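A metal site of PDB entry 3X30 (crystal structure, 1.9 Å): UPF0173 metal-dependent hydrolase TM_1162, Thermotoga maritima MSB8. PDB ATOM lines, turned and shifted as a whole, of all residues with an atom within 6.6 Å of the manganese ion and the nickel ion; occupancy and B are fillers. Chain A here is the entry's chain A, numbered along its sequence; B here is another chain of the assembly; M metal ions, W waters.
ND1 of His 109 lies close to O of Phe 168 (3.4 Å). The backbone NH (N) of His 191 sits at hydrogen-bond distance from the backbone carbonyl oxygen (O) of His 9, at 2.7 Å. The side-chain carboxylate (OD2) of Asp 53 sits close to a ring nitrogen (NE2) of His 9, at 2.7 Å.
His 9 touches the manganese ion. Five residues have an atom within 4 Å of the manganese ion: His 9, Asp 53, His 54, Asp 142 and His 191. Along chain A the residues within 4 Å of the manganese ion span positions 9 to 191. The nearest printed residue that does not touch the manganese ion is His 49 (4.3 Å).
Of the 15 residues printed, 4 come within 4 Å of the nickel ion. The nearest printed residue that does not touch the nickel ion is His 54 (4.1 Å).
The manganese ion is bound by OD2 of Asp 142 (2.1 Å), NE2 of His 54 (2.2 Å), water W3 (2.2 Å), NE2 of His 191 (2.3 Å), OD2 of Asp 53 (2.4 Å) and water W2 (2.4 Å). Slightly farther from the manganese ion lies the side-chain carboxylate (OD1) of Asp 142 (2.9 Å).
The nickel ion is bound by OD2 of Asp 142 (2.1 Å), NE2 of His 109 (2.1 Å), ND1 of His 51 (2.2 Å), NE2 of His 49 (2.2 Å), water W3 (2.2 Å) and water W1 (2.2 Å). The nickel ion has six donor atoms within binding distance.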
ATOM      1  N   HIS A   9     -24.213  27.439   7.867  1.00  0.00           N
ATOM      2  CA  HIS A   9     -23.160  27.052   6.916  1.00  0.00           C
ATOM      3  C   HIS A   9     -21.884  27.881   7.137  1.00  0.00           C
ATOM      4  O   HIS A   9     -21.184  27.664   8.119  1.00  0.00           O
ATOM      5  CB  HIS A   9     -23.656  27.135   5.465  1.00  0.00           C
ATOM      6  CG  HIS A   9     -22.876  26.267   4.523  1.00  0.00           C
ATOM      7  ND1 HIS A   9     -22.691  24.914   4.732  1.00  0.00           N
ATOM      8  CD2 HIS A   9     -22.219  26.562   3.371  1.00  0.00           C
ATOM      9  CE1 HIS A   9     -21.961  24.420   3.757  1.00  0.00           C
ATOM     10  NE2 HIS A   9     -21.662  25.389   2.910  1.00  0.00           N
ATOM     11  N   ALA A  10     -21.574  28.830   6.244  1.00  0.00           N
ATOM     12  CA  ALA A  10     -20.390  29.688   6.447  1.00  0.00           C
ATOM     13  C   ALA A  10     -20.760  31.176   6.500  1.00  0.00           C
ATOM     14  O   ALA A  10     -19.888  32.051   6.407  1.00  0.00           O
ATOM     15  CB  ALA A  10     -19.346  29.446   5.348  1.00  0.00           C
ATOM     16  N   HIS A  49     -14.346  32.190  -1.621  1.00  0.00           N
ATOM     17  CA  HIS A  49     -14.039  31.458  -2.845  1.00  0.00           C
ATOM     18  C   HIS A  49     -15.285  31.309  -3.704  1.00  0.00           C
ATOM     19  O   HIS A  49     -16.378  31.681  -3.285  1.00  0.00           O
ATOM     20  CB  HIS A  49     -13.391  30.090  -2.528  1.00  0.00           C
ATOM     21  CG  HIS A  49     -14.291  29.102  -1.834  1.00  0.00           C
ATOM     22  ND1 HIS A  49     -14.840  29.335  -0.586  1.00  0.00           N
ATOM     23  CD2 HIS A  49     -14.670  27.853  -2.177  1.00  0.00           C
ATOM     24  CE1 HIS A  49     -15.528  28.272  -0.202  1.00  0.00           C
ATOM     25  NE2 HIS A  49     -15.457  27.364  -1.164  1.00  0.00           N
ATOM     26  N   HIS A  51     -17.179  28.814  -4.895  1.00  0.00           N
ATOM     27  CA  HIS A  51     -18.212  27.778  -4.734  1.00  0.00           C
ATOM     28  C   HIS A  51     -19.549  28.400  -4.328  1.00  0.00           C
ATOM     29  O   HIS A  51     -19.598  29.347  -3.521  1.00  0.00           O
ATOM     30  CB  HIS A  51     -17.767  26.731  -3.697  1.00  0.00           C
ATOM     31  CG  HIS A  51     -16.578  25.933  -4.132  1.00  0.00           C
ATOM     32  ND1 HIS A  51     -15.841  25.149  -3.275  1.00  0.00           N
ATOM     33  CD2 HIS A  51     -15.983  25.817  -5.349  1.00  0.00           C
ATOM     34  CE1 HIS A  51     -14.841  24.590  -3.931  1.00  0.00           C
ATOM     35  NE2 HIS A  51     -14.901  24.985  -5.193  1.00  0.00           N
ATOM     36  N   ASP A  53     -22.070  27.801  -2.478  1.00  0.00           N
ATOM     37  CA  ASP A  53     -22.529  27.839  -1.083  1.00  0.00           C
ATOM     38  C   ASP A  53     -21.756  28.883  -0.277  1.00  0.00           C
ATOM     39  O   ASP A  53     -21.889  28.963   0.951  1.00  0.00           O
ATOM     40  CB  ASP A  53     -22.413  26.454  -0.430  1.00  0.00           C
ATOM     41  CG  ASP A  53     -21.022  25.840  -0.532  1.00  0.00           C
ATOM     42  OD1 ASP A  53     -20.392  25.896  -1.621  1.00  0.00           O
ATOM     43  OD2 ASP A  53     -20.545  25.299   0.491  1.00  0.00           O
ATOM     44  N   HIS A  54     -20.967  29.705  -0.975  1.00  0.00           N
ATOM     45  CA  HIS A  54     -20.231  30.805  -0.344  1.00  0.00           C
ATOM     46  C   HIS A  54     -20.469  32.091  -1.107  1.00  0.00           C
ATOM     47  O   HIS A  54     -20.866  33.087  -0.520  1.00  0.00           O
ATOM     48  CB  HIS A  54     -18.749  30.489  -0.256  1.00  0.00           C
ATOM     49  CG  HIS A  54     -18.463  29.292   0.593  1.00  0.00           C
ATOM     50  ND1 HIS A  54     -18.048  29.389   1.900  1.00  0.00           N
ATOM     51  CD2 HIS A  54     -18.627  27.971   0.338  1.00  0.00           C
ATOM     52  CE1 HIS A  54     -17.936  28.170   2.416  1.00  0.00           C
ATOM     53  NE2 HIS A  54     -18.283  27.299   1.486  1.00  0.00           N
ATOM     54  N   HIS A 109      -7.856  24.527  -0.862  1.00  0.00           N
ATOM     55  CA  HIS A 109      -9.223  24.245  -1.289  1.00  0.00           C
ATOM     56  C   HIS A 109      -9.276  24.471  -2.805  1.00  0.00           C
ATOM     57  O   HIS A 109      -8.233  24.384  -3.474  1.00  0.00           O
ATOM     58  CB  HIS A 109     -10.226  25.158  -0.518  1.00  0.00           C
ATOM     59  CG  HIS A 109     -11.660  24.745  -0.623  1.00  0.00           C
ATOM     60  ND1 HIS A 109     -12.140  23.565  -0.101  1.00  0.00           N
ATOM     61  CD2 HIS A 109     -12.735  25.370  -1.171  1.00  0.00           C
ATOM     62  CE1 HIS A 109     -13.441  23.475  -0.333  1.00  0.00           C
ATOM     63  NE2 HIS A 109     -13.825  24.558  -0.983  1.00  0.00           N
ATOM     64  N   GLY A 110     -10.457  24.761  -3.343  1.00  0.00           N
ATOM     65  CA  GLY A 110     -10.584  25.141  -4.743  1.00  0.00           C
ATOM     66  C   GLY A 110     -11.442  26.380  -4.860  1.00  0.00           C
ATOM     67  O   GLY A 110     -11.998  26.840  -3.861  1.00  0.00           O
ATOM     68  N   ASP A 142     -13.586  27.911   3.222  1.00  0.00           N
ATOM     69  CA  ASP A 142     -13.399  26.465   3.091  1.00  0.00           C
ATOM     70  C   ASP A 142     -11.910  26.180   3.008  1.00  0.00           C
ATOM     71  O   ASP A 142     -11.201  26.773   2.205  1.00  0.00           O
ATOM     72  CB  ASP A 142     -14.065  25.898   1.853  1.00  0.00           C
ATOM     73  CG  ASP A 142     -15.554  25.650   2.011  1.00  0.00           C
ATOM     74  OD1 ASP A 142     -16.111  25.836   3.113  1.00  0.00           O
ATOM     75  OD2 ASP A 142     -16.159  25.268   0.983  1.00  0.00           O
ATOM     76  N   PHE A 168     -15.295  18.040   2.258  1.00  0.00           N
ATOM     77  CA  PHE A 168     -14.844  19.199   1.475  1.00  0.00           C
ATOM     78  C   PHE A 168     -13.895  20.077   2.277  1.00  0.00           C
ATOM     79  O   PHE A 168     -13.156  20.888   1.696  1.00  0.00           O
ATOM     80  CB  PHE A 168     -16.004  20.064   1.012  1.00  0.00           C
ATOM     81  CG  PHE A 168     -16.935  19.364   0.061  1.00  0.00           C
ATOM     82  CD1 PHE A 168     -16.526  19.028  -1.213  1.00  0.00           C
ATOM     83  CD2 PHE A 168     -18.222  19.024   0.459  1.00  0.00           C
ATOM     84  CE1 PHE A 168     -17.387  18.376  -2.098  1.00  0.00           C
ATOM     85  CE2 PHE A 168     -19.083  18.384  -0.412  1.00  0.00           C
ATOM     86  CZ  PHE A 168     -18.670  18.057  -1.687  1.00  0.00           C
ATOM     87  N   VAL A 169     -13.937  19.945   3.589  1.00  0.00           N
ATOM     88  CA  VAL A 169     -13.182  20.805   4.496  1.00  0.00           C
ATOM     89  C   VAL A 169     -12.669  19.982   5.658  1.00  0.00           C
ATOM     90  O   VAL A 169     -12.967  18.787   5.739  1.00  0.00           O
ATOM     91  CB  VAL A 169     -14.048  21.964   5.043  1.00  0.00           C
ATOM     92  CG1 VAL A 169     -14.564  22.852   3.891  1.00  0.00           C
ATOM     93  CG2 VAL A 169     -15.202  21.404   5.860  1.00  0.00           C
ATOM     94  N   HIS A 191     -19.791  25.479   8.944  1.00  0.00           N
ATOM     95  CA  HIS A 191     -19.779  24.628   7.761  1.00  0.00           C
ATOM     96  C   HIS A 191     -19.960  23.165   8.157  1.00  0.00           C
ATOM     97  O   HIS A 191     -19.174  22.296   7.781  1.00  0.00           O
ATOM     98  CB  HIS A 191     -18.464  24.830   6.976  1.00  0.00           C
ATOM     99  CG  HIS A 191     -18.558  24.462   5.530  1.00  0.00           C
ATOM    100  ND1 HIS A 191     -18.470  23.160   5.070  1.00  0.00           N
ATOM    101  CD2 HIS A 191     -18.720  25.237   4.428  1.00  0.00           C
ATOM    102  CE1 HIS A 191     -18.570  23.147   3.753  1.00  0.00           C
ATOM    103  NE2 HIS A 191     -18.722  24.403   3.341  1.00  0.00           N
ATOM    104  N   TRP A 195     -25.764  19.804   5.129  1.00  0.00           N
ATOM    105  CA  TRP A 195     -26.173  18.586   4.421  1.00  0.00           C
ATOM    106  C   TRP A 195     -25.587  17.382   5.151  1.00  0.00           C
ATOM    107  O   TRP A 195     -24.670  17.528   5.953  1.00  0.00           O
ATOM    108  CB  TRP A 195     -25.711  18.613   2.957  1.00  0.00           C
ATOM    109  CG  TRP A 195     -26.246  19.778   2.213  1.00  0.00           C
ATOM    110  CD1 TRP A 195     -27.507  19.928   1.701  1.00  0.00           C
ATOM    111  CD2 TRP A 195     -25.534  20.975   1.876  1.00  0.00           C
ATOM    112  NE1 TRP A 195     -27.620  21.146   1.077  1.00  0.00           N
ATOM    113  CE2 TRP A 195     -26.421  21.805   1.163  1.00  0.00           C
ATOM    114  CE3 TRP A 195     -24.228  21.412   2.094  1.00  0.00           C
ATOM    115  CZ2 TRP A 195     -26.054  23.058   0.678  1.00  0.00           C
ATOM    116  CZ3 TRP A 195     -23.861  22.665   1.609  1.00  0.00           C
ATOM    117  CH2 TRP A 195     -24.763  23.460   0.914  1.00  0.00           C
ATOM    118  N   TYR B  73     -13.868  18.832  -6.157  1.00  0.00           N
ATOM    119  CA  TYR B  73     -15.173  19.224  -6.636  1.00  0.00           C
ATOM    120  C   TYR B  73     -15.164  19.548  -8.123  1.00  0.00           C
ATOM    121  O   TYR B  73     -16.033  19.106  -8.869  1.00  0.00           O
ATOM    122  CB  TYR B  73     -15.663  20.417  -5.806  1.00  0.00           C
ATOM    123  CG  TYR B  73     -16.884  21.147  -6.328  1.00  0.00           C
ATOM    124  CD1 TYR B  73     -18.147  20.581  -6.250  1.00  0.00           C
ATOM    125  CD2 TYR B  73     -16.765  22.438  -6.835  1.00  0.00           C
ATOM    126  CE1 TYR B  73     -19.270  21.288  -6.696  1.00  0.00           C
ATOM    127  CE2 TYR B  73     -17.854  23.133  -7.281  1.00  0.00           C
ATOM    128  CZ  TYR B  73     -19.101  22.561  -7.214  1.00  0.00           C
ATOM    129  OH  TYR B  73     -20.172  23.301  -7.679  1.00  0.00           O
ATOM    130  N   HIS B  90     -12.558  17.851  -1.197  1.00  0.00           N
ATOM    131  CA  HIS B  90     -11.567  18.869  -1.549  1.00  0.00           C
ATOM    132  C   HIS B  90     -10.387  18.829  -0.582  1.00  0.00           C
ATOM    133  O   HIS B  90     -10.331  17.970   0.315  1.00  0.00           O
ATOM    134  CB  HIS B  90     -12.163  20.288  -1.642  1.00  0.00           C
ATOM    135  CG  HIS B  90     -11.672  21.023  -2.863  1.00  0.00           C
ATOM    136  ND1 HIS B  90     -12.522  21.446  -3.866  1.00  0.00           N
ATOM    137  CD2 HIS B  90     -10.420  21.275  -3.296  1.00  0.00           C
ATOM    138  CE1 HIS B  90     -11.811  21.988  -4.834  1.00  0.00           C
ATOM    139  NE2 HIS B  90     -10.534  21.883  -4.523  1.00  0.00           N
HETATM  140 MN    MN M   1     -18.273  25.134   1.237  1.00  0.00          MN
HETATM  141 NI    NI M   2     -15.860  25.201  -1.120  1.00  0.00          NI
HETATM  142  O   HOH W   1     -16.449  23.050  -1.070  1.00  0.00           O
HETATM  143  O   HOH W   2     -18.289  22.790   0.732  1.00  0.00           O
HETATM  144  O   HOH W   3     -18.070  25.213  -0.991  1.00  0.00           O
